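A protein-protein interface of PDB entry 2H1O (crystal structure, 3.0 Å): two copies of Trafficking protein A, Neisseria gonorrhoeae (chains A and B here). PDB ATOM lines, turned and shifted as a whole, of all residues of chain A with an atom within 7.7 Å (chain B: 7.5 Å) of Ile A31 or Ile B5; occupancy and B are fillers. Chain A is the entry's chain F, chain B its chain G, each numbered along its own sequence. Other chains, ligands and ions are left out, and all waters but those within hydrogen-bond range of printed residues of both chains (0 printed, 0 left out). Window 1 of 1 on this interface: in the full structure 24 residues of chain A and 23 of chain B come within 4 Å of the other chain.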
ATOM      1  N   ALA A   1      -4.838  -9.158 -19.748  1.00  0.00           N
ATOM      2  CA  ALA A   1      -5.084  -9.343 -18.289  1.00  0.00           C
ATOM      3  C   ALA A   1      -5.673  -8.072 -17.690  1.00  0.00           C
ATOM      4  O   ALA A   1      -5.430  -6.971 -18.187  1.00  0.00           O
ATOM      5  CB  ALA A   1      -3.785  -9.704 -17.570  1.00  0.00           C
ATOM      6  N   SER A   2      -6.449  -8.225 -16.625  1.00  0.00           N
ATOM      7  CA  SER A   2      -7.056  -7.088 -15.965  1.00  0.00           C
ATOM      8  C   SER A   2      -6.321  -6.795 -14.677  1.00  0.00           C
ATOM      9  O   SER A   2      -5.752  -7.685 -14.073  1.00  0.00           O
ATOM     10  CB  SER A   2      -8.514  -7.387 -15.638  1.00  0.00           C
ATOM     11  OG  SER A   2      -9.349  -7.240 -16.765  1.00  0.00           O
ATOM     12  N   VAL A   3      -6.337  -5.544 -14.249  1.00  0.00           N
ATOM     13  CA  VAL A   3      -5.685  -5.162 -13.004  1.00  0.00           C
ATOM     14  C   VAL A   3      -6.426  -3.962 -12.433  1.00  0.00           C
ATOM     15  O   VAL A   3      -6.683  -2.992 -13.153  1.00  0.00           O
ATOM     16  CB  VAL A   3      -4.204  -4.794 -13.232  1.00  0.00           C
ATOM     17  CG1 VAL A   3      -3.664  -4.001 -12.052  1.00  0.00           C
ATOM     18  CG2 VAL A   3      -3.393  -6.053 -13.399  1.00  0.00           C
ATOM     19  N   VAL A   4      -6.773  -4.030 -11.147  1.00  0.00           N
ATOM     20  CA  VAL A   4      -7.494  -2.944 -10.495  1.00  0.00           C
ATOM     21  C   VAL A   4      -6.600  -2.195  -9.527  1.00  0.00           C
ATOM     22  O   VAL A   4      -5.988  -2.800  -8.652  1.00  0.00           O
ATOM     23  CB  VAL A   4      -8.703  -3.465  -9.693  1.00  0.00           C
ATOM     24  CG1 VAL A   4      -9.499  -2.304  -9.147  1.00  0.00           C
ATOM     25  CG2 VAL A   4      -9.566  -4.338 -10.561  1.00  0.00           C
ATOM     26  N   ILE A   5      -6.534  -0.879  -9.680  1.00  0.00           N
ATOM     27  CA  ILE A   5      -5.727  -0.053  -8.801  1.00  0.00           C
ATOM     28  C   ILE A   5      -6.673   0.785  -7.940  1.00  0.00           C
ATOM     29  O   ILE A   5      -7.354   1.696  -8.436  1.00  0.00           O
ATOM     30  CB  ILE A   5      -4.806   0.901  -9.605  1.00  0.00           C
ATOM     31  CG1 ILE A   5      -4.131   0.156 -10.751  1.00  0.00           C
ATOM     32  CG2 ILE A   5      -3.741   1.490  -8.693  1.00  0.00           C
ATOM     33  CD1 ILE A   5      -3.336  -1.023 -10.293  1.00  0.00           C
ATOM     34  N   LEU A   8      -5.904   5.112  -5.059  1.00  0.00           N
ATOM     35  CA  LEU A   8      -4.909   5.845  -5.805  1.00  0.00           C
ATOM     36  C   LEU A   8      -5.046   7.318  -5.438  1.00  0.00           C
ATOM     37  O   LEU A   8      -6.113   7.903  -5.568  1.00  0.00           O
ATOM     38  CB  LEU A   8      -5.155   5.654  -7.288  1.00  0.00           C
ATOM     39  CG  LEU A   8      -4.110   6.199  -8.246  1.00  0.00           C
ATOM     40  CD1 LEU A   8      -2.834   5.381  -8.124  1.00  0.00           C
ATOM     41  CD2 LEU A   8      -4.650   6.107  -9.662  1.00  0.00           C
ATOM     42  N   THR A  12      -2.183  12.046  -7.918  1.00  0.00           N
ATOM     43  CA  THR A  12      -1.486  11.127  -8.818  1.00  0.00           C
ATOM     44  C   THR A  12      -2.404  10.758  -9.985  1.00  0.00           C
ATOM     45  O   THR A  12      -1.957  10.612 -11.126  1.00  0.00           O
ATOM     46  CB  THR A  12      -1.035   9.837  -8.087  1.00  0.00           C
ATOM     47  OG1 THR A  12      -0.330   8.985  -9.000  1.00  0.00           O
ATOM     48  CG2 THR A  12      -2.219   9.086  -7.570  1.00  0.00           C
ATOM     49  N   HIS A  13      -3.695  10.633  -9.688  1.00  0.00           N
ATOM     50  CA  HIS A  13      -4.677  10.306 -10.704  1.00  0.00           C
ATOM     51  C   HIS A  13      -4.905  11.491 -11.646  1.00  0.00           C
ATOM     52  O   HIS A  13      -4.957  11.314 -12.861  1.00  0.00           O
ATOM     53  CB  HIS A  13      -5.984   9.893 -10.047  1.00  0.00           C
ATOM     54  CG  HIS A  13      -7.037   9.480 -11.022  1.00  0.00           C
ATOM     55  ND1 HIS A  13      -7.895  10.380 -11.615  1.00  0.00           N
ATOM     56  CD2 HIS A  13      -7.335   8.269 -11.547  1.00  0.00           C
ATOM     57  CE1 HIS A  13      -8.677   9.740 -12.465  1.00  0.00           C
ATOM     58  NE2 HIS A  13      -8.358   8.458 -12.444  1.00  0.00           N
ATOM     59  N   ILE A  16      -1.922  11.658 -14.032  1.00  0.00           N
ATOM     60  CA  ILE A  16      -1.914  10.660 -15.090  1.00  0.00           C
ATOM     61  C   ILE A  16      -2.980  11.037 -16.122  1.00  0.00           C
ATOM     62  O   ILE A  16      -2.745  11.012 -17.331  1.00  0.00           O
ATOM     63  CB  ILE A  16      -2.200   9.246 -14.517  1.00  0.00           C
ATOM     64  CG1 ILE A  16      -1.183   8.924 -13.428  1.00  0.00           C
ATOM     65  CG2 ILE A  16      -2.090   8.185 -15.600  1.00  0.00           C
ATOM     66  CD1 ILE A  16       0.247   8.920 -13.907  1.00  0.00           C
ATOM     67  N   LYS A  17      -4.154  11.406 -15.635  1.00  0.00           N
ATOM     68  CA  LYS A  17      -5.243  11.786 -16.512  1.00  0.00           C
ATOM     69  C   LYS A  17      -4.722  12.878 -17.437  1.00  0.00           C
ATOM     70  O   LYS A  17      -4.984  12.862 -18.636  1.00  0.00           O
ATOM     71  CB  LYS A  17      -6.418  12.284 -15.667  1.00  0.00           C
ATOM     72  CG  LYS A  17      -7.745  12.363 -16.394  1.00  0.00           C
ATOM     73  CD  LYS A  17      -8.876  12.669 -15.418  1.00  0.00           C
ATOM     74  CE  LYS A  17     -10.206  12.931 -16.130  1.00  0.00           C
ATOM     75  NZ  LYS A  17     -10.275  14.302 -16.738  1.00  0.00           N
ATOM     76  N   ALA A  20      -2.289  11.551 -20.188  1.00  0.00           N
ATOM     77  CA  ALA A  20      -3.078  10.826 -21.172  1.00  0.00           C
ATOM     78  C   ALA A  20      -3.742  11.748 -22.177  1.00  0.00           C
ATOM     79  O   ALA A  20      -3.532  11.627 -23.386  1.00  0.00           O
ATOM     80  CB  ALA A  20      -4.138   9.990 -20.467  1.00  0.00           C
ATOM     81  N   ARG A  25      -4.673  10.392 -25.376  1.00  0.00           N
ATOM     82  CA  ARG A  25      -4.956   9.015 -25.012  1.00  0.00           C
ATOM     83  C   ARG A  25      -5.959   8.986 -23.884  1.00  0.00           C
ATOM     84  O   ARG A  25      -6.114   9.956 -23.145  1.00  0.00           O
ATOM     85  CB  ARG A  25      -3.698   8.295 -24.539  1.00  0.00           C
ATOM     86  CG  ARG A  25      -2.530   8.332 -25.489  1.00  0.00           C
ATOM     87  CD  ARG A  25      -1.568   7.180 -25.229  1.00  0.00           C
ATOM     88  NE  ARG A  25      -0.214   7.517 -25.661  1.00  0.00           N
ATOM     89  CZ  ARG A  25       0.563   8.403 -25.041  1.00  0.00           C
ATOM     90  NH1 ARG A  25       0.124   9.037 -23.965  1.00  0.00           N
ATOM     91  NH2 ARG A  25       1.778   8.663 -25.499  1.00  0.00           N
ATOM     92  N   SER A  26      -6.645   7.860 -23.762  1.00  0.00           N
ATOM     93  CA  SER A  26      -7.609   7.654 -22.691  1.00  0.00           C
ATOM     94  C   SER A  26      -6.754   7.370 -21.477  1.00  0.00           C
ATOM     95  O   SER A  26      -5.682   6.791 -21.615  1.00  0.00           O
ATOM     96  CB  SER A  26      -8.457   6.425 -22.987  1.00  0.00           C
ATOM     97  OG  SER A  26      -7.621   5.295 -23.184  1.00  0.00           O
ATOM     98  N   THR A  27      -7.196   7.744 -20.287  1.00  0.00           N
ATOM     99  CA  THR A  27      -6.345   7.468 -19.147  1.00  0.00           C
ATOM    100  C   THR A  27      -5.972   6.000 -19.102  1.00  0.00           C
ATOM    101  O   THR A  27      -4.813   5.650 -18.909  1.00  0.00           O
ATOM    102  CB  THR A  27      -6.989   7.845 -17.833  1.00  0.00           C
ATOM    103  OG1 THR A  27      -7.198   9.260 -17.803  1.00  0.00           O
ATOM    104  CG2 THR A  27      -6.077   7.466 -16.686  1.00  0.00           C
ATOM    105  N   GLU A  28      -6.938   5.125 -19.309  1.00  0.00           N
ATOM    106  CA  GLU A  28      -6.601   3.728 -19.263  1.00  0.00           C
ATOM    107  C   GLU A  28      -5.439   3.376 -20.200  1.00  0.00           C
ATOM    108  O   GLU A  28      -4.508   2.685 -19.803  1.00  0.00           O
ATOM    109  CB  GLU A  28      -7.825   2.881 -19.579  1.00  0.00           C
ATOM    110  CG  GLU A  28      -7.518   1.401 -19.520  1.00  0.00           C
ATOM    111  CD  GLU A  28      -8.751   0.537 -19.545  1.00  0.00           C
ATOM    112  OE1 GLU A  28      -8.585  -0.701 -19.635  1.00  0.00           O
ATOM    113  OE2 GLU A  28      -9.875   1.091 -19.465  1.00  0.00           O
ATOM    114  N   ALA A  29      -5.473   3.855 -21.438  1.00  0.00           N
ATOM    115  CA  ALA A  29      -4.403   3.536 -22.380  1.00  0.00           C
ATOM    116  C   ALA A  29      -3.067   4.076 -21.896  1.00  0.00           C
ATOM    117  O   ALA A  29      -2.021   3.450 -22.091  1.00  0.00           O
ATOM    118  CB  ALA A  29      -4.719   4.104 -23.718  1.00  0.00           C
ATOM    119  N   GLU A  30      -3.111   5.250 -21.271  1.00  0.00           N
ATOM    120  CA  GLU A  30      -1.920   5.895 -20.726  1.00  0.00           C
ATOM    121  C   GLU A  30      -1.214   4.953 -19.736  1.00  0.00           C
ATOM    122  O   GLU A  30      -0.051   4.613 -19.912  1.00  0.00           O
ATOM    123  CB  GLU A  30      -2.335   7.199 -20.028  1.00  0.00           C
ATOM    124  CG  GLU A  30      -1.215   7.996 -19.391  1.00  0.00           C
ATOM    125  CD  GLU A  30      -0.109   8.354 -20.371  1.00  0.00           C
ATOM    126  OE1 GLU A  30      -0.416   8.566 -21.569  1.00  0.00           O
ATOM    127  OE2 GLU A  30       1.068   8.438 -19.936  1.00  0.00           O
ATOM    128  N   ILE A  31      -1.930   4.527 -18.702  1.00  0.00           N
ATOM    129  CA  ILE A  31      -1.370   3.636 -17.696  1.00  0.00           C
ATOM    130  C   ILE A  31      -0.837   2.372 -18.347  1.00  0.00           C
ATOM    131  O   ILE A  31       0.234   1.869 -18.007  1.00  0.00           O
ATOM    132  CB  ILE A  31      -2.435   3.247 -16.642  1.00  0.00           C
ATOM    133  CG1 ILE A  31      -2.885   4.497 -15.895  1.00  0.00           C
ATOM    134  CG2 ILE A  31      -1.873   2.225 -15.668  1.00  0.00           C
ATOM    135  CD1 ILE A  31      -3.994   4.258 -14.925  1.00  0.00           C
ATOM    136  N   ARG A  32      -1.601   1.864 -19.294  1.00  0.00           N
ATOM    137  CA  ARG A  32      -1.235   0.655 -20.021  1.00  0.00           C
ATOM    138  C   ARG A  32       0.128   0.863 -20.724  1.00  0.00           C
ATOM    139  O   ARG A  32       0.980  -0.029 -20.749  1.00  0.00           O
ATOM    140  CB  ARG A  32      -2.355   0.359 -21.024  1.00  0.00           C
ATOM    141  CG  ARG A  32      -2.386  -1.018 -21.590  1.00  0.00           C
ATOM    142  CD  ARG A  32      -3.437  -1.067 -22.688  1.00  0.00           C
ATOM    143  NE  ARG A  32      -4.802  -1.093 -22.163  1.00  0.00           N
ATOM    144  CZ  ARG A  32      -5.782  -0.295 -22.585  1.00  0.00           C
ATOM    145  NH1 ARG A  32      -5.545   0.608 -23.533  1.00  0.00           N
ATOM    146  NH2 ARG A  32      -7.009  -0.421 -22.086  1.00  0.00           N
ATOM    147  N   LEU A  33       0.332   2.053 -21.275  1.00  0.00           N
ATOM    148  CA  LEU A  33       1.574   2.358 -21.960  1.00  0.00           C
ATOM    149  C   LEU A  33       2.689   2.456 -20.945  1.00  0.00           C
ATOM    150  O   LEU A  33       3.754   1.881 -21.106  1.00  0.00           O
ATOM    151  CB  LEU A  33       1.453   3.677 -22.699  1.00  0.00           C
ATOM    152  CG  LEU A  33       2.746   4.148 -23.350  1.00  0.00           C
ATOM    153  CD1 LEU A  33       3.084   3.206 -24.476  1.00  0.00           C
ATOM    154  CD2 LEU A  33       2.594   5.589 -23.844  1.00  0.00           C
ATOM    155  N   ILE A  34       2.439   3.207 -19.890  1.00  0.00           N
ATOM    156  CA  ILE A  34       3.420   3.370 -18.844  1.00  0.00           C
ATOM    157  C   ILE A  34       3.924   2.013 -18.404  1.00  0.00           C
ATOM    158  O   ILE A  34       5.094   1.706 -18.577  1.00  0.00           O
ATOM    159  CB  ILE A  34       2.818   4.119 -17.673  1.00  0.00           C
ATOM    160  CG1 ILE A  34       2.537   5.560 -18.112  1.00  0.00           C
ATOM    161  CG2 ILE A  34       3.731   4.034 -16.493  1.00  0.00           C
ATOM    162  CD1 ILE A  34       2.016   6.451 -17.026  1.00  0.00           C
ATOM    163  N   LEU A  35       3.042   1.189 -17.860  1.00  0.00           N
ATOM    164  CA  LEU A  35       3.439  -0.142 -17.425  1.00  0.00           C
ATOM    165  C   LEU A  35       4.171  -0.881 -18.540  1.00  0.00           C
ATOM    166  O   LEU A  35       5.082  -1.660 -18.276  1.00  0.00           O
ATOM    167  CB  LEU A  35       2.213  -0.934 -16.979  1.00  0.00           C
ATOM    168  CG  LEU A  35       1.871  -0.855 -15.487  1.00  0.00           C
ATOM    169  CD1 LEU A  35       2.296   0.467 -14.883  1.00  0.00           C
ATOM    170  CD2 LEU A  35       0.393  -1.085 -15.311  1.00  0.00           C
ATOM    171  N   ASP A  36       3.781  -0.623 -19.788  1.00  0.00           N
ATOM    172  CA  ASP A  36       4.428  -1.253 -20.938  1.00  0.00           C
ATOM    173  C   ASP A  36       5.860  -0.838 -21.079  1.00  0.00           C
ATOM    174  O   ASP A  36       6.721  -1.661 -21.324  1.00  0.00           O
ATOM    175  CB  ASP A  36       3.731  -0.880 -22.221  1.00  0.00           C
ATOM    176  CG  ASP A  36       2.712  -1.889 -22.623  1.00  0.00           C
ATOM    177  OD1 ASP A  36       2.218  -1.805 -23.778  1.00  0.00           O
ATOM    178  OD2 ASP A  36       2.405  -2.768 -21.781  1.00  0.00           O
ATOM    179  N   ASN A  37       6.112   0.456 -20.944  1.00  0.00           N
ATOM    180  CA  ASN A  37       7.468   0.963 -21.064  1.00  0.00           C
ATOM    181  C   ASN A  37       8.373   0.413 -19.976  1.00  0.00           C
ATOM    182  O   ASN A  37       9.520   0.052 -20.229  1.00  0.00           O
ATOM    183  CB  ASN A  37       7.449   2.492 -21.067  1.00  0.00           C
ATOM    184  CG  ASN A  37       7.021   3.045 -22.419  1.00  0.00           C
ATOM    185  OD1 ASN A  37       7.626   2.721 -23.441  1.00  0.00           O
ATOM    186  ND2 ASN A  37       5.975   3.861 -22.436  1.00  0.00           N
ATOM    187  N   ILE A  38       7.840   0.325 -18.769  1.00  0.00           N
ATOM    188  CA  ILE A  38       8.600  -0.215 -17.669  1.00  0.00           C
ATOM    189  C   ILE A  38       9.024  -1.644 -17.986  1.00  0.00           C
ATOM    190  O   ILE A  38      10.186  -1.999 -17.829  1.00  0.00           O
ATOM    191  CB  ILE A  38       7.776  -0.151 -16.403  1.00  0.00           C
ATOM    192  CG1 ILE A  38       7.897   1.256 -15.837  1.00  0.00           C
ATOM    193  CG2 ILE A  38       8.228  -1.202 -15.405  1.00  0.00           C
ATOM    194  CD1 ILE A  38       7.093   1.482 -14.605  1.00  0.00           C
ATOM    195  N   SER B   2     -10.070   4.771  -8.149  1.00  0.00           N
ATOM    196  CA  SER B   2      -9.879   3.411  -8.631  1.00  0.00           C
ATOM    197  C   SER B   2      -9.783   3.492 -10.143  1.00  0.00           C
ATOM    198  O   SER B   2     -10.208   4.477 -10.747  1.00  0.00           O
ATOM    199  CB  SER B   2     -11.086   2.540  -8.278  1.00  0.00           C
ATOM    200  OG  SER B   2     -11.244   2.371  -6.885  1.00  0.00           O
ATOM    201  N   VAL B   3      -9.217   2.466 -10.758  1.00  0.00           N
ATOM    202  CA  VAL B   3      -9.105   2.414 -12.214  1.00  0.00           C
ATOM    203  C   VAL B   3      -8.867   0.967 -12.543  1.00  0.00           C
ATOM    204  O   VAL B   3      -8.162   0.277 -11.810  1.00  0.00           O
ATOM    205  CB  VAL B   3      -7.890   3.187 -12.766  1.00  0.00           C
ATOM    206  CG1 VAL B   3      -8.004   4.655 -12.460  1.00  0.00           C
ATOM    207  CG2 VAL B   3      -6.628   2.632 -12.172  1.00  0.00           C
ATOM    208  N   VAL B   4      -9.465   0.485 -13.623  1.00  0.00           N
ATOM    209  CA  VAL B   4      -9.230  -0.892 -14.013  1.00  0.00           C
ATOM    210  C   VAL B   4      -8.503  -0.858 -15.348  1.00  0.00           C
ATOM    211  O   VAL B   4      -8.902  -0.163 -16.282  1.00  0.00           O
ATOM    212  CB  VAL B   4     -10.535  -1.690 -14.144  1.00  0.00           C
ATOM    213  CG1 VAL B   4     -11.448  -1.030 -15.148  1.00  0.00           C
ATOM    214  CG2 VAL B   4     -10.228  -3.116 -14.564  1.00  0.00           C
ATOM    215  N   ILE B   5      -7.403  -1.582 -15.421  1.00  0.00           N
ATOM    216  CA  ILE B   5      -6.642  -1.612 -16.637  1.00  0.00           C
ATOM    217  C   ILE B   5      -6.930  -2.928 -17.330  1.00  0.00           C
ATOM    218  O   ILE B   5      -6.414  -3.979 -16.956  1.00  0.00           O
ATOM    219  CB  ILE B   5      -5.130  -1.423 -16.338  1.00  0.00           C
ATOM    220  CG1 ILE B   5      -4.828   0.065 -16.148  1.00  0.00           C
ATOM    221  CG2 ILE B   5      -4.285  -1.922 -17.488  1.00  0.00           C
ATOM    222  CD1 ILE B   5      -5.773   0.777 -15.221  1.00  0.00           C
ATOM    223  N   ARG B   6      -7.791  -2.861 -18.335  1.00  0.00           N
ATOM    224  CA  ARG B   6      -8.158  -4.043 -19.091  1.00  0.00           C
ATOM    225  C   ARG B   6      -7.253  -4.193 -20.299  1.00  0.00           C
ATOM    226  O   ARG B   6      -6.675  -3.224 -20.794  1.00  0.00           O
ATOM    227  CB  ARG B   6      -9.626  -3.958 -19.518  1.00  0.00           C
ATOM    228  CG  ARG B   6     -10.606  -4.249 -18.378  1.00  0.00           C
ATOM    229  CD  ARG B   6     -11.917  -3.499 -18.529  1.00  0.00           C
ATOM    230  NE  ARG B   6     -11.723  -2.054 -18.465  1.00  0.00           N
ATOM    231  CZ  ARG B   6     -12.694  -1.184 -18.198  1.00  0.00           C
ATOM    232  NH1 ARG B   6     -13.929  -1.615 -17.963  1.00  0.00           N
ATOM    233  NH2 ARG B   6     -12.435   0.121 -18.177  1.00  0.00           N
ATOM    234  N   ASN B   7      -7.130  -5.425 -20.767  1.00  0.00           N
ATOM    235  CA  ASN B   7      -6.285  -5.726 -21.908  1.00  0.00           C
ATOM    236  C   ASN B   7      -4.851  -5.315 -21.657  1.00  0.00           C
ATOM    237  O   ASN B   7      -4.294  -4.512 -22.400  1.00  0.00           O
ATOM    238  CB  ASN B   7      -6.806  -5.031 -23.160  1.00  0.00           C
ATOM    239  CG  ASN B   7      -8.118  -5.613 -23.635  1.00  0.00           C
ATOM    240  OD1 ASN B   7      -8.252  -6.832 -23.755  1.00  0.00           O
ATOM    241  ND2 ASN B   7      -9.096  -4.747 -23.912  1.00  0.00           N
ATOM    242  N   LEU B   8      -4.263  -5.860 -20.594  1.00  0.00           N
ATOM    243  CA  LEU B   8      -2.874  -5.593 -20.247  1.00  0.00           C
ATOM    244  C   LEU B   8      -2.161  -6.880 -20.663  1.00  0.00           C
ATOM    245  O   LEU B   8      -2.493  -7.942 -20.152  1.00  0.00           O
ATOM    246  CB  LEU B   8      -2.749  -5.386 -18.739  1.00  0.00           C
ATOM    247  CG  LEU B   8      -1.749  -4.350 -18.227  1.00  0.00           C
ATOM    248  CD1 LEU B   8      -1.710  -4.370 -16.705  1.00  0.00           C
ATOM    249  CD2 LEU B   8      -0.389  -4.652 -18.770  1.00  0.00           C
ATOM    250  N   SER B   9      -1.212  -6.811 -21.595  1.00  0.00           N
ATOM    251  CA  SER B   9      -0.517  -8.025 -22.037  1.00  0.00           C
ATOM    252  C   SER B   9       0.094  -8.808 -20.874  1.00  0.00           C
ATOM    253  O   SER B   9       0.707  -8.228 -19.978  1.00  0.00           O
ATOM    254  CB  SER B   9       0.587  -7.682 -23.024  1.00  0.00           C
ATOM    255  OG  SER B   9       1.650  -7.025 -22.361  1.00  0.00           O
ATOM    256  N   THR B  12       3.764  -7.770 -20.087  1.00  0.00           N
ATOM    257  CA  THR B  12       3.886  -6.588 -19.256  1.00  0.00           C
ATOM    258  C   THR B  12       3.445  -6.921 -17.853  1.00  0.00           C
ATOM    259  O   THR B  12       4.092  -6.556 -16.876  1.00  0.00           O
ATOM    260  CB  THR B  12       2.979  -5.478 -19.748  1.00  0.00           C
ATOM    261  OG1 THR B  12       3.250  -5.228 -21.131  1.00  0.00           O
ATOM    262  CG2 THR B  12       3.194  -4.201 -18.924  1.00  0.00           C
ATOM    263  N   ILE B  31       2.101  -0.593  -8.818  1.00  0.00           N
ATOM    264  CA  ILE B  31       1.548   0.286  -9.840  1.00  0.00           C
ATOM    265  C   ILE B  31       1.236   1.637  -9.226  1.00  0.00           C
ATOM    266  O   ILE B  31       1.513   2.701  -9.806  1.00  0.00           O
ATOM    267  CB  ILE B  31       0.280  -0.319 -10.487  1.00  0.00           C
ATOM    268  CG1 ILE B  31       0.676  -1.521 -11.346  1.00  0.00           C
ATOM    269  CG2 ILE B  31      -0.403   0.716 -11.374  1.00  0.00           C
ATOM    270  CD1 ILE B  31      -0.481  -2.348 -11.875  1.00  0.00           C
ATOM    271  N   ILE B  34       4.586   3.328  -9.054  1.00  0.00           N
ATOM    272  CA  ILE B  34       5.060   3.691 -10.369  1.00  0.00           C
ATOM    273  C   ILE B  34       4.326   4.930 -10.842  1.00  0.00           C
ATOM    274  O   ILE B  34       4.943   5.885 -11.330  1.00  0.00           O
ATOM    275  CB  ILE B  34       4.828   2.548 -11.358  1.00  0.00           C
ATOM    276  CG1 ILE B  34       5.756   1.376 -11.008  1.00  0.00           C
ATOM    277  CG2 ILE B  34       5.037   3.041 -12.777  1.00  0.00           C
ATOM    278  CD1 ILE B  34       5.668   0.187 -11.944  1.00  0.00           C
ATOM    279  N   LEU B  35       3.004   4.916 -10.698  1.00  0.00           N
ATOM    280  CA  LEU B  35       2.196   6.054 -11.095  1.00  0.00           C
ATOM    281  C   LEU B  35       2.530   7.259 -10.226  1.00  0.00           C
ATOM    282  O   LEU B  35       2.727   8.357 -10.736  1.00  0.00           O
ATOM    283  CB  LEU B  35       0.721   5.718 -10.963  1.00  0.00           C
ATOM    284  CG  LEU B  35       0.214   4.729 -12.008  1.00  0.00           C
ATOM    285  CD1 LEU B  35      -1.243   4.401 -11.742  1.00  0.00           C
ATOM    286  CD2 LEU B  35       0.387   5.322 -13.394  1.00  0.00           C
ATOM    287  N   ILE B  38       5.600   9.080 -11.252  1.00  0.00           N
ATOM    288  CA  ILE B  38       5.377   9.807 -12.483  1.00  0.00           C
ATOM    289  C   ILE B  38       4.630  11.086 -12.167  1.00  0.00           C
ATOM    290  O   ILE B  38       5.014  12.175 -12.600  1.00  0.00           O
ATOM    291  CB  ILE B  38       4.574   8.964 -13.453  1.00  0.00           C
ATOM    292  CG1 ILE B  38       5.504   7.945 -14.110  1.00  0.00           C
ATOM    293  CG2 ILE B  38       3.854   9.856 -14.441  1.00  0.00           C
ATOM    294  CD1 ILE B  38       4.781   6.857 -14.835  1.00  0.00           C
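The backbone NH (N) of Asn B7 sits at hydrogen-bond distance from the backbone carbonyl oxygen (O) of Ala A1, 3.5 Å away.
The backbone NH of Ala A1 is in hydrogen-bond range of the backbone carbonyl oxygen of Leu B8 (2.7 Å).
N of Ile B5 sits at hydrogen-bond distance from O of Val A3, 2.8 Å away.
N of Ile A5 sits at hydrogen-bond distance from O of Val B3, at 2.9 Å.
OE2 of Glu A28 lies within salt-bridge range of NH2 of Arg B6 (3.0 Å).
NH2 of Arg A32 lies within hydrogen-bond range of O of Arg B6 (3.1 Å).
NE of Arg A32 sits at hydrogen-bond distance from O of Asn B7 (3.5 Å).
OD2 of Asp A36 is in hydrogen-bond range of OG1 of Thr B12, 2.7 Å away.
The backbone carbonyl oxygen (O) of Ala A1 lies close to the backbone carbonyl oxygen (O) of Ile B5, at 3.4 Å.
O of Val B4 sits close to OE1 of Glu A28.
NH2 of Arg A32 is in salt-bridge range of OE1 of Glu A28 (2.9 Å).
The side-chain hydroxyl (OG1) of Thr B12 is in hydrogen-bond range of the side-chain hydroxyl (OG) of Ser B9, at 2.7 Å.
Among the printed residues, pairs that only touch across the chains: Ala A1 with Arg B6 (3.9 Å), Ser A2 with Ile B5 (3.3 Å), Ser A2 with Arg B6 (3.6 Å), Val A3 with Val B3 (3.8 Å), Val A3 with Val B4 (3.4 Å), Val A3 with Ile B31 (3.6 Å), Val A4 with Val B3 (3.5 Å), Ile A5 with Ser B2 (3.1 Å), Ile A5 with Ile B31 (3.5 Å), Thr A12 with Leu B35 (3.6 Å), His A13 with Val B3 (3.8 Å), Ile A16 with Leu B35 (3.6 Å), Ile A16 with Ile B38 (3.8 Å), Glu A28 with Ile B5 (3.6 Å), Ile A31 with Ile B5 (3.7 Å), Ile A34 with Ile B38 (3.4 Å), Leu A35 with Thr B12 (3.2 Å), Leu A35 with Ile B31 (3.8 Å) and Ile A38 with Ile B34 (3.2 Å).
Of the printed residues of chain B, Ile A5 touches Ser B2 (3.1 Å), Val B3 (2.9 Å) and Ile B31 (3.5 Å).
Lys A17 touches none of the printed residues of chain B.
Ile A31 touches just one residue of chain B: Ile B5 (3.7 Å).
Printed residues of chain B within 4 Å of Ile A38: Ile B34.
The nearest printed residue of chain B that does not touch Ala A1 is Ser B9 (4.7 Å).
Of the 13 printed residues of chain B, 12 touch a printed residue of chain A.
Printed residues of chain B that touch a printed residue of chain A: Ser B2, Val B3, Val B4, Ile B5, Arg B6, Asn B7, Leu B8, Thr B12, Ile B31, Ile B34, Leu B35 and Ile B38.
Hydrophobic or aromatic side chains of chain B that line the printed part of chain A: Val B3, Val B4, Ile B5, Leu B8, Ile B31, Ile B34, Leu B35 and Ile B38.
Of the 25 printed residues of chain A, 15 touch a printed residue of chain B.
Hydrophobic or aromatic side chains of chain A within 4 Å of the printed part of chain B: Ala A1, Val A3, Val A4, Ile A5, His A13, Ile A16, Ile A31, Ile A34, Leu A35 and Ile A38.
Among the printed residues, 29 pairs touch across the chains.
Ser A2 touches Ile B5, and with the chains exchanged Ile A5 touches Ser B2.
Val A3 touches Ile B31, but with the chains exchanged Ile A31 does not touch Val B3 (4.1 Å).
Ile A5 touches Ile B31, and with the chains exchanged Ile A31 touches Ile B5.
Ile A34 touches Ile B38, and with the chains exchanged Ile A38 touches Ile B34.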
